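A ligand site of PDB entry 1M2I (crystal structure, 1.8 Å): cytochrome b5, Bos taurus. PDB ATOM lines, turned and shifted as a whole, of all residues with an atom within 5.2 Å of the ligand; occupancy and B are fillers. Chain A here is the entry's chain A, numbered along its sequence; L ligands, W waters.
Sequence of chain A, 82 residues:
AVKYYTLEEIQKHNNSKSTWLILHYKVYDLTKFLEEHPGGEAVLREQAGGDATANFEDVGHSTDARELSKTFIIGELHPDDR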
ATOM      1  N   LEU A  21      23.954 -11.162  -4.008  1.00  0.00           N
ATOM      2  CA  LEU A  21      25.160 -11.101  -3.202  1.00  0.00           C
ATOM      3  C   LEU A  21      24.866 -11.776  -1.883  1.00  0.00           C
ATOM      4  O   LEU A  21      23.713 -11.991  -1.534  1.00  0.00           O
ATOM      5  CB  LEU A  21      25.661  -9.662  -3.011  1.00  0.00           C
ATOM      6  CG  LEU A  21      24.874  -8.399  -2.660  1.00  0.00           C
ATOM      7  CD1 LEU A  21      24.481  -8.397  -1.192  1.00  0.00           C
ATOM      8  CD2 LEU A  21      25.753  -7.194  -2.963  1.00  0.00           C
ATOM      9  N   LEU A  23      25.366 -11.947   2.334  1.00  0.00           N
ATOM     10  CA  LEU A  23      25.659 -11.191   3.549  1.00  0.00           C
ATOM     11  C   LEU A  23      25.303 -12.091   4.714  1.00  0.00           C
ATOM     12  O   LEU A  23      24.152 -12.498   4.853  1.00  0.00           O
ATOM     13  CB  LEU A  23      24.808  -9.916   3.635  1.00  0.00           C
ATOM     14  CG  LEU A  23      25.006  -8.795   2.617  1.00  0.00           C
ATOM     15  CD1 LEU A  23      23.964  -7.707   2.869  1.00  0.00           C
ATOM     16  CD2 LEU A  23      26.398  -8.221   2.734  1.00  0.00           C
ATOM     17  N   TYR A  28      20.826 -12.374  -1.014  1.00  0.00           N
ATOM     18  CA  TYR A  28      19.974 -11.227  -1.303  1.00  0.00           C
ATOM     19  C   TYR A  28      19.874 -10.945  -2.788  1.00  0.00           C
ATOM     20  O   TYR A  28      20.880 -10.959  -3.487  1.00  0.00           O
ATOM     21  CB  TYR A  28      20.509  -9.961  -0.621  1.00  0.00           C
ATOM     22  CG  TYR A  28      20.566 -10.036   0.889  1.00  0.00           C
ATOM     23  CD1 TYR A  28      21.544 -10.816   1.529  1.00  0.00           C
ATOM     24  CD2 TYR A  28      19.632  -9.377   1.673  1.00  0.00           C
ATOM     25  CE1 TYR A  28      21.574 -10.928   2.905  1.00  0.00           C
ATOM     26  CE2 TYR A  28      19.654  -9.486   3.061  1.00  0.00           C
ATOM     27  CZ  TYR A  28      20.626 -10.269   3.671  1.00  0.00           C
ATOM     28  OH  TYR A  28      20.622 -10.410   5.035  1.00  0.00           O
ATOM     29  N   LEU A  30      19.305  -8.107  -5.077  1.00  0.00           N
ATOM     30  CA  LEU A  30      19.239  -6.650  -5.070  1.00  0.00           C
ATOM     31  C   LEU A  30      18.990  -6.016  -6.431  1.00  0.00           C
ATOM     32  O   LEU A  30      19.176  -4.812  -6.608  1.00  0.00           O
ATOM     33  CB  LEU A  30      20.531  -6.066  -4.497  1.00  0.00           C
ATOM     34  CG  LEU A  30      20.929  -6.524  -3.094  1.00  0.00           C
ATOM     35  CD1 LEU A  30      22.185  -5.755  -2.663  1.00  0.00           C
ATOM     36  CD2 LEU A  30      19.791  -6.269  -2.125  1.00  0.00           C
ATOM     37  N   PHE A  33      16.886  -2.940  -6.325  1.00  0.00           N
ATOM     38  CA  PHE A  33      17.292  -2.014  -5.276  1.00  0.00           C
ATOM     39  C   PHE A  33      18.491  -1.178  -5.739  1.00  0.00           C
ATOM     40  O   PHE A  33      18.802  -0.134  -5.159  1.00  0.00           O
ATOM     41  CB  PHE A  33      17.647  -2.819  -4.014  1.00  0.00           C
ATOM     42  CG  PHE A  33      18.079  -1.982  -2.848  1.00  0.00           C
ATOM     43  CD1 PHE A  33      19.390  -2.051  -2.376  1.00  0.00           C
ATOM     44  CD2 PHE A  33      17.180  -1.136  -2.207  1.00  0.00           C
ATOM     45  CE1 PHE A  33      19.789  -1.290  -1.276  1.00  0.00           C
ATOM     46  CE2 PHE A  33      17.572  -0.372  -1.113  1.00  0.00           C
ATOM     47  CZ  PHE A  33      18.876  -0.453  -0.642  1.00  0.00           C
ATOM     48  N   HIS A  37      19.568   2.404  -3.773  1.00  0.00           N
ATOM     49  CA  HIS A  37      20.616   2.348  -2.758  1.00  0.00           C
ATOM     50  C   HIS A  37      21.319   3.688  -2.524  1.00  0.00           C
ATOM     51  O   HIS A  37      21.957   4.220  -3.427  1.00  0.00           O
ATOM     52  CB  HIS A  37      21.643   1.280  -3.136  1.00  0.00           C
ATOM     53  CG  HIS A  37      22.730   1.107  -2.131  1.00  0.00           C
ATOM     54  ND1 HIS A  37      24.076   1.108  -2.437  1.00  0.00           N
ATOM     55  CD2 HIS A  37      22.651   0.894  -0.793  1.00  0.00           C
ATOM     56  CE1 HIS A  37      24.754   0.897  -1.307  1.00  0.00           C
ATOM     57  NE2 HIS A  37      23.936   0.758  -0.284  1.00  0.00           N
ATOM     58  N   PRO A  38      21.217   4.227  -1.295  1.00  0.00           N
ATOM     59  CA  PRO A  38      21.851   5.510  -0.959  1.00  0.00           C
ATOM     60  C   PRO A  38      23.351   5.541  -1.246  1.00  0.00           C
ATOM     61  O   PRO A  38      23.904   6.583  -1.585  1.00  0.00           O
ATOM     62  CB  PRO A  38      21.552   5.663   0.532  1.00  0.00           C
ATOM     63  CG  PRO A  38      20.220   4.982   0.671  1.00  0.00           C
ATOM     64  CD  PRO A  38      20.413   3.732  -0.171  1.00  0.00           C
ATOM     65  N   GLY A  39      23.998   4.388  -1.108  1.00  0.00           N
ATOM     66  CA  GLY A  39      25.424   4.312  -1.359  1.00  0.00           C
ATOM     67  C   GLY A  39      25.767   4.127  -2.822  1.00  0.00           C
ATOM     68  O   GLY A  39      26.935   3.959  -3.163  1.00  0.00           O
ATOM     69  N   VAL A  43      28.787   0.280  -6.010  1.00  0.00           N
ATOM     70  CA  VAL A  43      29.353  -0.486  -4.903  1.00  0.00           C
ATOM     71  C   VAL A  43      28.664  -1.848  -4.779  1.00  0.00           C
ATOM     72  O   VAL A  43      29.246  -2.799  -4.251  1.00  0.00           O
ATOM     73  CB  VAL A  43      29.199   0.275  -3.554  1.00  0.00           C
ATOM     74  CG1 VAL A  43      27.737   0.364  -3.159  1.00  0.00           C
ATOM     75  CG2 VAL A  43      30.004  -0.431  -2.479  1.00  0.00           C
ATOM     76  N   LEU A  44      27.445  -1.954  -5.281  1.00  0.00           N
ATOM     77  CA  LEU A  44      26.710  -3.208  -5.234  1.00  0.00           C
ATOM     78  C   LEU A  44      27.103  -4.127  -6.380  1.00  0.00           C
ATOM     79  O   LEU A  44      27.327  -5.316  -6.185  1.00  0.00           O
ATOM     80  CB  LEU A  44      25.199  -2.941  -5.252  1.00  0.00           C
ATOM     81  CG  LEU A  44      24.689  -2.122  -4.064  1.00  0.00           C
ATOM     82  CD1 LEU A  44      23.174  -1.929  -4.166  1.00  0.00           C
ATOM     83  CD2 LEU A  44      25.041  -2.847  -2.775  1.00  0.00           C
ATOM     84  N   GLN A  47      30.336  -6.092  -5.967  1.00  0.00           N
ATOM     85  CA  GLN A  47      30.309  -7.233  -5.060  1.00  0.00           C
ATOM     86  C   GLN A  47      29.364  -8.339  -5.544  1.00  0.00           C
ATOM     87  O   GLN A  47      29.350  -9.442  -4.982  1.00  0.00           O
ATOM     88  CB  GLN A  47      29.857  -6.789  -3.661  1.00  0.00           C
ATOM     89  CG  GLN A  47      30.786  -5.810  -2.980  1.00  0.00           C
ATOM     90  CD  GLN A  47      32.167  -6.387  -2.713  1.00  0.00           C
ATOM     91  OE1 GLN A  47      32.302  -7.472  -2.133  1.00  0.00           O
ATOM     92  NE2 GLN A  47      33.201  -5.667  -3.117  1.00  0.00           N
ATOM     93  N   ALA A  52      29.730 -10.180   0.373  1.00  0.00           N
ATOM     94  CA  ALA A  52      30.056  -8.786   0.615  1.00  0.00           C
ATOM     95  C   ALA A  52      29.903  -8.414   2.092  1.00  0.00           C
ATOM     96  O   ALA A  52      29.841  -7.237   2.446  1.00  0.00           O
ATOM     97  CB  ALA A  52      29.144  -7.889  -0.222  1.00  0.00           C
ATOM     98  N   ASN A  55      32.562  -5.797   3.609  1.00  0.00           N
ATOM     99  CA  ASN A  55      32.368  -4.451   3.097  1.00  0.00           C
ATOM    100  C   ASN A  55      31.103  -3.817   3.648  1.00  0.00           C
ATOM    101  O   ASN A  55      31.055  -2.619   3.910  1.00  0.00           O
ATOM    102  CB  ASN A  55      32.294  -4.462   1.565  1.00  0.00           C
ATOM    103  CG  ASN A  55      33.416  -5.250   0.945  1.00  0.00           C
ATOM    104  OD1 ASN A  55      33.409  -6.477   0.947  1.00  0.00           O
ATOM    105  ND2 ASN A  55      34.408  -4.535   0.413  1.00  0.00           N
ATOM    106  N   PHE A  56      30.074  -4.634   3.834  1.00  0.00           N
ATOM    107  CA  PHE A  56      28.788  -4.172   4.361  1.00  0.00           C
ATOM    108  C   PHE A  56      28.949  -3.675   5.791  1.00  0.00           C
ATOM    109  O   PHE A  56      28.445  -2.610   6.151  1.00  0.00           O
ATOM    110  CB  PHE A  56      27.772  -5.323   4.325  1.00  0.00           C
ATOM    111  CG  PHE A  56      26.412  -4.958   4.859  1.00  0.00           C
ATOM    112  CD1 PHE A  56      25.494  -4.259   4.067  1.00  0.00           C
ATOM    113  CD2 PHE A  56      26.035  -5.331   6.144  1.00  0.00           C
ATOM    114  CE1 PHE A  56      24.228  -3.941   4.553  1.00  0.00           C
ATOM    115  CE2 PHE A  56      24.769  -5.014   6.648  1.00  0.00           C
ATOM    116  CZ  PHE A  56      23.858  -4.319   5.843  1.00  0.00           C
ATOM    117  N   VAL A  59      31.282  -0.287   6.339  1.00  0.00           N
ATOM    118  CA  VAL A  59      30.691   1.050   6.243  1.00  0.00           C
ATOM    119  C   VAL A  59      29.731   1.276   7.407  1.00  0.00           C
ATOM    120  O   VAL A  59      29.247   2.392   7.620  1.00  0.00           O
ATOM    121  CB  VAL A  59      29.915   1.232   4.915  1.00  0.00           C
ATOM    122  CG1 VAL A  59      30.771   0.775   3.736  1.00  0.00           C
ATOM    123  CG2 VAL A  59      28.623   0.455   4.970  1.00  0.00           C
ATOM    124  N   GLY A  60      29.460   0.220   8.156  1.00  0.00           N
ATOM    125  CA  GLY A  60      28.591   0.310   9.321  1.00  0.00           C
ATOM    126  C   GLY A  60      27.125   0.704   9.157  1.00  0.00           C
ATOM    127  O   GLY A  60      26.654   1.644   9.796  1.00  0.00           O
ATOM    128  N   HIS A  61      26.413  -0.039   8.312  1.00  0.00           N
ATOM    129  CA  HIS A  61      25.015   0.268   8.035  1.00  0.00           C
ATOM    130  C   HIS A  61      24.177   0.433   9.283  1.00  0.00           C
ATOM    131  O   HIS A  61      24.421  -0.224  10.297  1.00  0.00           O
ATOM    132  CB  HIS A  61      24.395  -0.826   7.158  1.00  0.00           C
ATOM    133  CG  HIS A  61      24.820  -0.767   5.728  1.00  0.00           C
ATOM    134  ND1 HIS A  61      26.035  -1.210   5.254  1.00  0.00           N
ATOM    135  CD2 HIS A  61      24.178  -0.226   4.663  1.00  0.00           C
ATOM    136  CE1 HIS A  61      26.083  -0.935   3.947  1.00  0.00           C
ATOM    137  NE2 HIS A  61      24.984  -0.333   3.549  1.00  0.00           N
ATOM    138  N   SER A  62      23.187   1.308   9.208  1.00  0.00           N
ATOM    139  CA  SER A  62      22.303   1.600  10.324  1.00  0.00           C
ATOM    140  C   SER A  62      21.277   0.506  10.573  1.00  0.00           C
ATOM    141  O   SER A  62      21.161  -0.440   9.795  1.00  0.00           O
ATOM    142  CB  SER A  62      21.564   2.918  10.065  1.00  0.00           C
ATOM    143  OG  SER A  62      20.722   2.799   8.927  1.00  0.00           O
ATOM    144  N   ALA A  65      18.677   0.379   7.811  1.00  0.00           N
ATOM    145  CA  ALA A  65      19.214  -0.246   6.601  1.00  0.00           C
ATOM    146  C   ALA A  65      19.161  -1.766   6.719  1.00  0.00           C
ATOM    147  O   ALA A  65      18.809  -2.461   5.766  1.00  0.00           O
ATOM    148  CB  ALA A  65      20.647   0.209   6.366  1.00  0.00           C
ATOM    149  N   LEU A  68      15.542  -3.100   6.501  1.00  0.00           N
ATOM    150  CA  LEU A  68      15.077  -3.063   5.116  1.00  0.00           C
ATOM    151  C   LEU A  68      15.683  -4.195   4.290  1.00  0.00           C
ATOM    152  O   LEU A  68      15.007  -4.781   3.440  1.00  0.00           O
ATOM    153  CB  LEU A  68      15.449  -1.722   4.477  1.00  0.00           C
ATOM    154  CG  LEU A  68      15.148  -1.559   2.987  1.00  0.00           C
ATOM    155  CD1 LEU A  68      13.650  -1.593   2.754  1.00  0.00           C
ATOM    156  CD2 LEU A  68      15.755  -0.259   2.479  1.00  0.00           C
ATOM    157  N   SER A  69      16.947  -4.510   4.538  1.00  0.00           N
ATOM    158  CA  SER A  69      17.628  -5.556   3.785  1.00  0.00           C
ATOM    159  C   SER A  69      16.903  -6.896   3.829  1.00  0.00           C
ATOM    160  O   SER A  69      16.943  -7.670   2.885  1.00  0.00           O
ATOM    161  CB  SER A  69      19.056  -5.736   4.293  1.00  0.00           C
ATOM    162  OG  SER A  69      19.065  -6.384   5.561  1.00  0.00           O
ATOM    163  N   PHE A  72      14.815  -8.343   0.938  1.00  0.00           N
ATOM    164  CA  PHE A  72      15.468  -8.852  -0.267  1.00  0.00           C
ATOM    165  C   PHE A  72      16.062 -10.256  -0.150  1.00  0.00           C
ATOM    166  O   PHE A  72      16.699 -10.745  -1.088  1.00  0.00           O
ATOM    167  CB  PHE A  72      16.562  -7.876  -0.689  1.00  0.00           C
ATOM    168  CG  PHE A  72      16.061  -6.482  -0.968  1.00  0.00           C
ATOM    169  CD1 PHE A  72      15.176  -6.246  -2.010  1.00  0.00           C
ATOM    170  CD2 PHE A  72      16.448  -5.415  -0.168  1.00  0.00           C
ATOM    171  CE1 PHE A  72      14.679  -4.960  -2.247  1.00  0.00           C
ATOM    172  CE2 PHE A  72      15.966  -4.129  -0.387  1.00  0.00           C
ATOM    173  CZ  PHE A  72      15.074  -3.906  -1.430  1.00  0.00           C
HETATM  174  C1  LIG L   1      24.649   3.494   2.630  1.00  0.00           C
HETATM  175  C2  LIG L   1      21.050   0.251   2.497  1.00  0.00           C
HETATM  176  C3  LIG L   1      24.145  -3.103   0.952  1.00  0.00           C
HETATM  177  C4  LIG L   1      27.678   0.223   0.661  1.00  0.00           C
HETATM  178  C5  LIG L   1      23.421   2.869   2.817  1.00  0.00           C
HETATM  179  C6  LIG L   1      22.263   3.484   3.449  1.00  0.00           C
HETATM  180  C7  LIG L   1      21.252   2.589   3.343  1.00  0.00           C
HETATM  181  C8  LIG L   1      21.788   1.414   2.700  1.00  0.00           C
HETATM  182  C9  LIG L   1      19.801   2.724   3.827  1.00  0.00           C
HETATM  183  C10 LIG L   1      22.208   4.826   4.179  1.00  0.00           C
HETATM  184  C11 LIG L   1      22.934   4.821   5.520  1.00  0.00           C
HETATM  185  C12 LIG L   1      22.371   3.806   6.495  1.00  0.00           C
HETATM  186  O1  LIG L   1      21.146   3.826   6.715  1.00  0.00           O
HETATM  187  O2  LIG L   1      23.146   2.994   7.035  1.00  0.00           O
HETATM  188  C13 LIG L   1      21.594  -0.952   2.055  1.00  0.00           C
HETATM  189  C14 LIG L   1      20.865  -2.188   1.964  1.00  0.00           C
HETATM  190  C15 LIG L   1      21.710  -3.116   1.476  1.00  0.00           C
HETATM  191  C16 LIG L   1      22.986  -2.463   1.353  1.00  0.00           C
HETATM  192  C17 LIG L   1      19.395  -2.421   2.318  1.00  0.00           C
HETATM  193  C18 LIG L   1      21.337  -4.380   1.015  1.00  0.00           C
HETATM  194  C19 LIG L   1      21.411  -5.560   1.764  1.00  0.00           C
HETATM  195  C20 LIG L   1      25.374  -2.496   0.804  1.00  0.00           C
HETATM  196  C21 LIG L   1      26.592  -3.217   0.429  1.00  0.00           C
HETATM  197  C22 LIG L   1      27.588  -2.288   0.293  1.00  0.00           C
HETATM  198  C23 LIG L   1      26.977  -0.997   0.617  1.00  0.00           C
HETATM  199  C24 LIG L   1      26.702  -4.721   0.206  1.00  0.00           C
HETATM  200  C25 LIG L   1      28.941  -2.467  -0.025  1.00  0.00           C
HETATM  201  C26 LIG L   1      29.567  -3.597  -0.573  1.00  0.00           C
HETATM  202  C27 LIG L   1      27.134   1.417   1.131  1.00  0.00           C
HETATM  203  C28 LIG L   1      27.812   2.700   1.125  1.00  0.00           C
HETATM  204  C29 LIG L   1      27.011   3.592   1.727  1.00  0.00           C
HETATM  205  C30 LIG L   1      25.778   2.891   2.063  1.00  0.00           C
HETATM  206  C31 LIG L   1      29.166   3.012   0.515  1.00  0.00           C
HETATM  207  C32 LIG L   1      27.398   5.028   2.098  1.00  0.00           C
HETATM  208  C33 LIG L   1      27.768   5.086   3.568  1.00  0.00           C
HETATM  209  C34 LIG L   1      28.135   6.488   4.029  1.00  0.00           C
HETATM  210  O3  LIG L   1      28.516   6.640   5.214  1.00  0.00           O
HETATM  211  O4  LIG L   1      28.050   7.422   3.206  1.00  0.00           O
HETATM  212  N1  LIG L   1      23.134   1.565   2.412  1.00  0.00           N
HETATM  213  N2  LIG L   1      22.918  -1.130   1.702  1.00  0.00           N
HETATM  214  N3  LIG L   1      25.630  -1.143   0.980  1.00  0.00           N
HETATM  215  N4  LIG L   1      25.847   1.553   1.656  1.00  0.00           N
HETATM  216 FE1  LIG L   1      24.379   0.213   1.693  1.00  0.00          FE
HETATM  217  O   HOH W   1      24.657   7.376   2.608  1.00  0.00           O
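A ring nitrogen (NE2) of His 61 is bound to an iron atom (FE1) of the ligand, at 2.0 Å.
An oxygen (O1) of the ligand is in hydrogen-bond range of the side-chain hydroxyl of Ser 62 (2.5 Å).
N of Ser 62 lies within hydrogen-bond range of O2 of the ligand (2.8 Å).
A ring nitrogen (NE2) of His 37 binds an iron atom (FE1) of the ligand.
OG of Ser 62 sits at hydrogen-bond distance from N of Ala 65 (3.4 Å).
The side-chain amide oxygen (OE1) of Gln 47 lies close to the side-chain amide oxygen (OD1) of Asn 55, at 3.4 Å.
ND1 of His 61 lies within hydrogen-bond range of O of Phe 56, at 2.9 Å.
Leu 23 touches the ligand.
CD2 of Leu 30 touches C18 of the ligand, at 3.98 Å.
CE1 of Phe 33 touches C14 of the ligand (3.5 Å).
Pro 38 touches the ligand (CB to C6, 3.7 Å).
Gly 39 touches the ligand (CA to C29, 3.5 Å).
Val 43 touches the ligand (CG2 to C25, 3.4 Å).
Leu 44 touches the ligand.
CG of Gln 47 touches C26 of the ligand (3.5 Å).
CB of Asn 55 touches C26 of the ligand (3.6 Å).
CD1 of Phe 56 touches C3 of the ligand, at 3.6 Å.
Ala 65 touches the ligand.
CB of Ser 69 touches C19 of the ligand, at 3.5 Å.
Hydrophobic or aromatic side chains that line the ligand: Leu 23, Leu 30, Phe 33, His 37, Pro 38, Val 43, Leu 44, Phe 56, His 61 and Ala 65.
15 residues have an atom within 4 Å of the ligand: Leu 23, Leu 30, Phe 33, His 37, Pro 38, Gly 39, Val 43, Leu 44, Gln 47, Asn 55, Phe 56, His 61, Ser 62, Ala 65 and Ser 69.
The nearest printed residue that does not touch the ligand is Ala 52 (4.02 Å).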
